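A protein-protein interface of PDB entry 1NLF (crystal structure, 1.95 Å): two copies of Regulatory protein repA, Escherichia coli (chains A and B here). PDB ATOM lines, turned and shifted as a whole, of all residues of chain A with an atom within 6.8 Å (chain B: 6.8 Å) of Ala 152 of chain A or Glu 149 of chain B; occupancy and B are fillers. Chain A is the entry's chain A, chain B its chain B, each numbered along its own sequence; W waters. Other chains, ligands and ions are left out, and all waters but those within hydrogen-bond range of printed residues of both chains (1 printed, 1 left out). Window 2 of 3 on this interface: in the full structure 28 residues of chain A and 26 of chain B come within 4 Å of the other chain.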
ATOM      1  N   GLU A 148     -22.458   2.206  -1.686  1.00  0.00           N
ATOM      2  CA  GLU A 148     -22.301   0.760  -1.770  1.00  0.00           C
ATOM      3  C   GLU A 148     -23.559   0.034  -1.319  1.00  0.00           C
ATOM      4  O   GLU A 148     -24.540   0.646  -0.891  1.00  0.00           O
ATOM      5  CB  GLU A 148     -21.139   0.277  -0.889  1.00  0.00           C
ATOM      6  CG  GLU A 148     -19.832   1.042  -1.018  1.00  0.00           C
ATOM      7  CD  GLU A 148     -19.339   1.154  -2.442  1.00  0.00           C
ATOM      8  OE1 GLU A 148     -19.487   0.171  -3.202  1.00  0.00           O
ATOM      9  OE2 GLU A 148     -18.791   2.229  -2.790  1.00  0.00           O
ATOM     10  N   GLU A 149     -23.503  -1.288  -1.418  1.00  0.00           N
ATOM     11  CA  GLU A 149     -24.582  -2.168  -1.001  1.00  0.00           C
ATOM     12  C   GLU A 149     -24.236  -2.452   0.465  1.00  0.00           C
ATOM     13  O   GLU A 149     -23.187  -3.034   0.745  1.00  0.00           O
ATOM     14  CB  GLU A 149     -24.515  -3.452  -1.830  1.00  0.00           C
ATOM     15  CG  GLU A 149     -25.843  -4.107  -2.122  1.00  0.00           C
ATOM     16  CD  GLU A 149     -26.808  -3.187  -2.846  1.00  0.00           C
ATOM     17  OE1 GLU A 149     -26.370  -2.411  -3.723  1.00  0.00           O
ATOM     18  OE2 GLU A 149     -28.015  -3.253  -2.541  1.00  0.00           O
ATOM     19  N   GLU A 150     -25.091  -2.036   1.399  1.00  0.00           N
ATOM     20  CA  GLU A 150     -24.799  -2.244   2.816  1.00  0.00           C
ATOM     21  C   GLU A 150     -24.796  -3.719   3.210  1.00  0.00           C
ATOM     22  O   GLU A 150     -24.511  -4.062   4.358  1.00  0.00           O
ATOM     23  CB  GLU A 150     -25.785  -1.452   3.700  1.00  0.00           C
ATOM     24  CG  GLU A 150     -25.764   0.061   3.440  1.00  0.00           C
ATOM     25  CD  GLU A 150     -26.358   0.900   4.579  1.00  0.00           C
ATOM     26  OE1 GLU A 150     -27.373   0.483   5.176  1.00  0.00           O
ATOM     27  OE2 GLU A 150     -25.814   1.992   4.865  1.00  0.00           O
ATOM     28  N   ASN A 151     -25.084  -4.583   2.239  1.00  0.00           N
ATOM     29  CA  ASN A 151     -25.126  -6.025   2.458  1.00  0.00           C
ATOM     30  C   ASN A 151     -23.836  -6.700   1.997  1.00  0.00           C
ATOM     31  O   ASN A 151     -23.633  -7.892   2.236  1.00  0.00           O
ATOM     32  CB  ASN A 151     -26.305  -6.631   1.693  1.00  0.00           C
ATOM     33  CG  ASN A 151     -27.589  -5.851   1.887  1.00  0.00           C
ATOM     34  OD1 ASN A 151     -28.091  -5.725   3.004  1.00  0.00           O
ATOM     35  ND2 ASN A 151     -28.127  -5.318   0.796  1.00  0.00           N
ATOM     36  N   ALA A 152     -22.977  -5.937   1.324  1.00  0.00           N
ATOM     37  CA  ALA A 152     -21.707  -6.460   0.825  1.00  0.00           C
ATOM     38  C   ALA A 152     -20.597  -6.188   1.842  1.00  0.00           C
ATOM     39  O   ALA A 152     -20.204  -5.041   2.057  1.00  0.00           O
ATOM     40  CB  ALA A 152     -21.375  -5.819  -0.517  1.00  0.00           C
ATOM     41  N   SER A 153     -20.094  -7.250   2.464  1.00  0.00           N
ATOM     42  CA  SER A 153     -19.059  -7.126   3.485  1.00  0.00           C
ATOM     43  C   SER A 153     -17.770  -6.478   3.017  1.00  0.00           C
ATOM     44  O   SER A 153     -17.131  -5.764   3.780  1.00  0.00           O
ATOM     45  CB  SER A 153     -18.739  -8.499   4.089  1.00  0.00           C
ATOM     46  OG  SER A 153     -18.198  -9.375   3.117  1.00  0.00           O
ATOM     47  N   GLY A 154     -17.380  -6.733   1.774  1.00  0.00           N
ATOM     48  CA  GLY A 154     -16.152  -6.151   1.262  1.00  0.00           C
ATOM     49  C   GLY A 154     -16.254  -4.642   1.152  1.00  0.00           C
ATOM     50  O   GLY A 154     -15.484  -3.910   1.778  1.00  0.00           O
ATOM     51  N   PRO A 155     -17.199  -4.143   0.345  1.00  0.00           N
ATOM     52  CA  PRO A 155     -17.368  -2.700   0.183  1.00  0.00           C
ATOM     53  C   PRO A 155     -17.597  -1.986   1.517  1.00  0.00           C
ATOM     54  O   PRO A 155     -17.073  -0.893   1.733  1.00  0.00           O
ATOM     55  CB  PRO A 155     -18.574  -2.603  -0.752  1.00  0.00           C
ATOM     56  CG  PRO A 155     -18.394  -3.810  -1.625  1.00  0.00           C
ATOM     57  CD  PRO A 155     -18.051  -4.882  -0.604  1.00  0.00           C
ATOM     58  N   MET A 156     -18.363  -2.602   2.413  1.00  0.00           N
ATOM     59  CA  MET A 156     -18.633  -1.972   3.701  1.00  0.00           C
ATOM     60  C   MET A 156     -17.408  -1.954   4.611  1.00  0.00           C
ATOM     61  O   MET A 156     -17.249  -1.045   5.432  1.00  0.00           O
ATOM     62  CB  MET A 156     -19.813  -2.651   4.401  1.00  0.00           C
ATOM     63  CG  MET A 156     -21.155  -2.408   3.703  1.00  0.00           C
ATOM     64  SD  MET A 156     -21.395  -0.676   3.180  1.00  0.00           S
ATOM     65  CE  MET A 156     -21.518   0.107   4.768  1.00  0.00           C
ATOM     66  N   ALA A 157     -16.540  -2.953   4.464  1.00  0.00           N
ATOM     67  CA  ALA A 157     -15.320  -2.997   5.258  1.00  0.00           C
ATOM     68  C   ALA A 157     -14.449  -1.809   4.834  1.00  0.00           C
ATOM     69  O   ALA A 157     -13.687  -1.270   5.638  1.00  0.00           O
ATOM     70  CB  ALA A 157     -14.575  -4.314   5.016  1.00  0.00           C
ATOM     71  N   VAL A 201     -22.469  -7.852   8.032  1.00  0.00           N
ATOM     72  CA  VAL A 201     -23.284  -6.667   8.266  1.00  0.00           C
ATOM     73  C   VAL A 201     -22.453  -5.525   8.846  1.00  0.00           C
ATOM     74  O   VAL A 201     -21.281  -5.695   9.180  1.00  0.00           O
ATOM     75  CB  VAL A 201     -24.448  -6.975   9.232  1.00  0.00           C
ATOM     76  CG1 VAL A 201     -25.437  -7.924   8.571  1.00  0.00           C
ATOM     77  CG2 VAL A 201     -23.905  -7.585  10.513  1.00  0.00           C
ATOM     78  N   ASN A 205     -18.710  -5.130  11.794  1.00  0.00           N
ATOM     79  CA  ASN A 205     -17.500  -4.336  11.595  1.00  0.00           C
ATOM     80  C   ASN A 205     -17.319  -3.211  12.609  1.00  0.00           C
ATOM     81  O   ASN A 205     -16.364  -2.439  12.516  1.00  0.00           O
ATOM     82  CB  ASN A 205     -17.487  -3.729  10.189  1.00  0.00           C
ATOM     83  CG  ASN A 205     -17.037  -4.713   9.129  1.00  0.00           C
ATOM     84  OD1 ASN A 205     -16.950  -4.366   7.953  1.00  0.00           O
ATOM     85  ND2 ASN A 205     -16.745  -5.943   9.539  1.00  0.00           N
ATOM     86  N   ARG B 143     -10.403 -10.046   8.823  1.00  0.00           N
ATOM     87  CA  ARG B 143     -11.320  -9.106   8.166  1.00  0.00           C
ATOM     88  C   ARG B 143     -10.697  -7.746   7.844  1.00  0.00           C
ATOM     89  O   ARG B 143     -11.098  -7.079   6.883  1.00  0.00           O
ATOM     90  CB  ARG B 143     -12.569  -8.905   9.040  1.00  0.00           C
ATOM     91  CG  ARG B 143     -13.666  -8.000   8.452  1.00  0.00           C
ATOM     92  CD  ARG B 143     -14.287  -8.551   7.156  1.00  0.00           C
ATOM     93  NE  ARG B 143     -13.575  -8.103   5.954  1.00  0.00           N
ATOM     94  CZ  ARG B 143     -14.006  -8.285   4.709  1.00  0.00           C
ATOM     95  NH1 ARG B 143     -15.156  -8.913   4.479  1.00  0.00           N
ATOM     96  NH2 ARG B 143     -13.295  -7.819   3.687  1.00  0.00           N
ATOM     97  N   HIS B 146      -8.063  -7.589   4.269  1.00  0.00           N
ATOM     98  CA  HIS B 146      -8.508  -7.782   2.891  1.00  0.00           C
ATOM     99  C   HIS B 146      -9.855  -7.091   2.685  1.00  0.00           C
ATOM    100  O   HIS B 146     -10.545  -6.762   3.656  1.00  0.00           O
ATOM    101  CB  HIS B 146      -8.595  -9.283   2.556  1.00  0.00           C
ATOM    102  CG  HIS B 146      -9.778  -9.976   3.152  1.00  0.00           C
ATOM    103  ND1 HIS B 146     -10.973 -10.117   2.479  1.00  0.00           N
ATOM    104  CD2 HIS B 146      -9.957 -10.558   4.362  1.00  0.00           C
ATOM    105  CE1 HIS B 146     -11.838 -10.753   3.249  1.00  0.00           C
ATOM    106  NE2 HIS B 146     -11.248 -11.032   4.397  1.00  0.00           N
ATOM    107  N   ILE B 147     -10.221  -6.844   1.428  1.00  0.00           N
ATOM    108  CA  ILE B 147     -11.489  -6.183   1.131  1.00  0.00           C
ATOM    109  C   ILE B 147     -12.428  -7.059   0.305  1.00  0.00           C
ATOM    110  O   ILE B 147     -13.283  -6.552  -0.424  1.00  0.00           O
ATOM    111  CB  ILE B 147     -11.262  -4.843   0.377  1.00  0.00           C
ATOM    112  CG1 ILE B 147     -10.606  -5.101  -0.979  1.00  0.00           C
ATOM    113  CG2 ILE B 147     -10.373  -3.925   1.210  1.00  0.00           C
ATOM    114  CD1 ILE B 147     -10.519  -3.863  -1.869  1.00  0.00           C
ATOM    115  N   GLU B 148     -12.284  -8.375   0.436  1.00  0.00           N
ATOM    116  CA  GLU B 148     -13.116  -9.304  -0.328  1.00  0.00           C
ATOM    117  C   GLU B 148     -14.302  -9.843   0.459  1.00  0.00           C
ATOM    118  O   GLU B 148     -14.487  -9.532   1.638  1.00  0.00           O
ATOM    119  CB  GLU B 148     -12.287 -10.503  -0.806  1.00  0.00           C
ATOM    120  CG  GLU B 148     -10.944 -10.168  -1.423  1.00  0.00           C
ATOM    121  CD  GLU B 148     -11.056  -9.276  -2.641  1.00  0.00           C
ATOM    122  OE1 GLU B 148     -11.974  -9.495  -3.460  1.00  0.00           O
ATOM    123  OE2 GLU B 148     -10.213  -8.362  -2.779  1.00  0.00           O
ATOM    124  N   GLU B 149     -15.099 -10.663  -0.219  1.00  0.00           N
ATOM    125  CA  GLU B 149     -16.258 -11.311   0.378  1.00  0.00           C
ATOM    126  C   GLU B 149     -15.686 -12.611   0.946  1.00  0.00           C
ATOM    127  O   GLU B 149     -15.167 -13.432   0.191  1.00  0.00           O
ATOM    128  CB  GLU B 149     -17.286 -11.618  -0.712  1.00  0.00           C
ATOM    129  CG  GLU B 149     -18.710 -11.205  -0.401  1.00  0.00           C
ATOM    130  CD  GLU B 149     -18.834  -9.743  -0.012  1.00  0.00           C
ATOM    131  OE1 GLU B 149     -18.179  -8.889  -0.644  1.00  0.00           O
ATOM    132  OE2 GLU B 149     -19.604  -9.448   0.923  1.00  0.00           O
ATOM    133  N   GLU B 150     -15.775 -12.807   2.260  1.00  0.00           N
ATOM    134  CA  GLU B 150     -15.206 -14.008   2.870  1.00  0.00           C
ATOM    135  C   GLU B 150     -15.941 -15.297   2.521  1.00  0.00           C
ATOM    136  O   GLU B 150     -15.451 -16.394   2.804  1.00  0.00           O
ATOM    137  CB  GLU B 150     -15.106 -13.841   4.398  1.00  0.00           C
ATOM    138  CG  GLU B 150     -14.308 -12.604   4.820  1.00  0.00           C
ATOM    139  CD  GLU B 150     -13.917 -12.595   6.297  1.00  0.00           C
ATOM    140  OE1 GLU B 150     -14.752 -12.973   7.149  1.00  0.00           O
ATOM    141  OE2 GLU B 150     -12.772 -12.192   6.605  1.00  0.00           O
ATOM    142  N   ASN B 151     -17.109 -15.161   1.898  1.00  0.00           N
ATOM    143  CA  ASN B 151     -17.901 -16.313   1.492  1.00  0.00           C
ATOM    144  C   ASN B 151     -17.668 -16.626   0.012  1.00  0.00           C
ATOM    145  O   ASN B 151     -18.311 -17.509  -0.555  1.00  0.00           O
ATOM    146  CB  ASN B 151     -19.388 -16.051   1.749  1.00  0.00           C
ATOM    147  CG  ASN B 151     -19.892 -14.802   1.049  1.00  0.00           C
ATOM    148  OD1 ASN B 151     -19.876 -14.714  -0.178  1.00  0.00           O
ATOM    149  ND2 ASN B 151     -20.344 -13.829   1.830  1.00  0.00           N
ATOM    150  N   ALA B 152     -16.749 -15.890  -0.608  1.00  0.00           N
ATOM    151  CA  ALA B 152     -16.418 -16.096  -2.017  1.00  0.00           C
ATOM    152  C   ALA B 152     -15.121 -16.897  -2.106  1.00  0.00           C
ATOM    153  O   ALA B 152     -14.043 -16.382  -1.800  1.00  0.00           O
ATOM    154  CB  ALA B 152     -16.254 -14.755  -2.713  1.00  0.00           C
ATOM    155  N   SER B 153     -15.227 -18.152  -2.536  1.00  0.00           N
ATOM    156  CA  SER B 153     -14.067 -19.038  -2.629  1.00  0.00           C
ATOM    157  C   SER B 153     -12.925 -18.547  -3.510  1.00  0.00           C
ATOM    158  O   SER B 153     -11.761 -18.722  -3.161  1.00  0.00           O
ATOM    159  CB  SER B 153     -14.501 -20.433  -3.102  1.00  0.00           C
ATOM    160  OG  SER B 153     -14.955 -20.408  -4.446  1.00  0.00           O
ATOM    161  N   PRO B 155     -11.950 -15.291  -4.465  1.00  0.00           N
ATOM    162  CA  PRO B 155     -11.227 -14.196  -3.814  1.00  0.00           C
ATOM    163  C   PRO B 155     -10.470 -14.622  -2.560  1.00  0.00           C
ATOM    164  O   PRO B 155      -9.316 -14.248  -2.376  1.00  0.00           O
ATOM    165  CB  PRO B 155     -12.334 -13.191  -3.516  1.00  0.00           C
ATOM    166  CG  PRO B 155     -13.249 -13.375  -4.687  1.00  0.00           C
ATOM    167  CD  PRO B 155     -13.333 -14.887  -4.776  1.00  0.00           C
ATOM    168  N   MET B 156     -11.113 -15.399  -1.695  1.00  0.00           N
ATOM    169  CA  MET B 156     -10.453 -15.839  -0.469  1.00  0.00           C
ATOM    170  C   MET B 156      -9.303 -16.798  -0.747  1.00  0.00           C
ATOM    171  O   MET B 156      -8.390 -16.928   0.069  1.00  0.00           O
ATOM    172  CB  MET B 156     -11.457 -16.486   0.488  1.00  0.00           C
ATOM    173  CG  MET B 156     -12.495 -15.510   1.026  1.00  0.00           C
ATOM    174  SD  MET B 156     -11.752 -13.957   1.582  1.00  0.00           S
ATOM    175  CE  MET B 156     -10.801 -14.517   2.930  1.00  0.00           C
HETATM  176  O   HOH W   1     -17.795 -11.806   4.105  1.00  0.00           O
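Of chain B, only Glu 149 (3.5 Å) comes within 4 Å of Ala 152 of chain A.
Of the printed residues of chain B, Ala 157 of chain A touches Arg 143 (3.96 Å).
Of the printed residues of chain B, Asn 205 of chain A touches Arg 143 (3.9 Å).
Of the printed residues of chain B, Ser 153 of chain A touches Arg 143 (3.4 Å), Glu 148 (3.998 Å) and Glu 149 (2.6 Å).
Printed residues of chain B within 4 Å of Gly 154 of chain A: Ile 147, Glu 148 and Glu 149.
Printed residues of chain A within 4 Å of Arg 143 of chain B: Ser 153, Ala 157 and Asn 205.
Glu 148 of chain A touches none of the printed residues of chain B.
The nearest residue of chain B that does not touch Ala 152 of chain A is Arg 143 of chain B (6.6 Å).
The nearest printed residue of chain A that does not touch Glu 149 of chain B is Pro 155 of chain A (4.01 Å).
Ala 152 of chain A touches Glu 149 of chain B, but with the chains exchanged Glu 149 of chain A does not touch Ala 152 of chain B (14.0 Å).
Ser 153 of chain A touches Glu 148 of chain B, but with the chains exchanged Glu 148 of chain A does not touch Ser 153 of chain B (18.8 Å).
Ser 153 of chain A touches Glu 149 of chain B, but with the chains exchanged Glu 149 of chain A does not touch Ser 153 of chain B (17.4 Å).
OG of Ser 153 of chain A lies within hydrogen-bond range of NH1 of Arg 143 of chain B, at 3.4 Å.
The side-chain hydroxyl (OG) of Ser 153 of chain A sits at hydrogen-bond distance from the side-chain carboxylate (OE2) of Glu 149 of chain B, at 2.6 Å.
The backbone NH (N) of Gly 154 of chain A sits at hydrogen-bond distance from the side-chain carboxylate (OE1) of Glu 149 of chain B (3.3 Å).
Of the 11 printed residues of chain B, 4 touch a printed residue of chain A.
Of the 12 printed residues of chain A, 5 touch a printed residue of chain B.
Hydrophobic or aromatic side chains of chain A that line the printed part of chain B: Ala 157.
Among the printed residues, 9 pairs touch across the chains.
Among the printed residues, no Asp or Glu carboxylate lies within 4 Å of a Lys or Arg side-chain nitrogen of the other chain.
The guanidinium group of Arg 143 of chain B lies within hydrogen-bond range of the backbone carbonyl oxygen of His 146 of chain B (2.9 Å).
The guanidinium group (NH2) of Arg 143 of chain B lies within hydrogen-bond range of the backbone carbonyl oxygen (O) of Glu 148 of chain B, at 2.9 Å.
A ring nitrogen (ND1) of His 146 of chain B lies within hydrogen-bond range of the backbone NH (N) of Glu 148 of chain B.
Among the printed residues, merely in contact across the chains: Gly 154 of chain A with Ile 147 of chain B (3.4 Å), Ala 152 of chain A with Glu 149 of chain B (3.5 Å), Gly 154 of chain A with Glu 148 of chain B (3.8 Å), Asn 205 of chain A with Arg 143 of chain B (3.9 Å), Ala 157 of chain A with Arg 143 of chain B (3.96 Å) and Ser 153 of chain A with Glu 148 of chain B (3.998 Å).
Water W1 lies within hydrogen-bond range of the side-chain hydroxyl of Ser 153 of chain A (2.7 Å) and the backbone NH of Glu 150 of chain B (2.9 Å).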
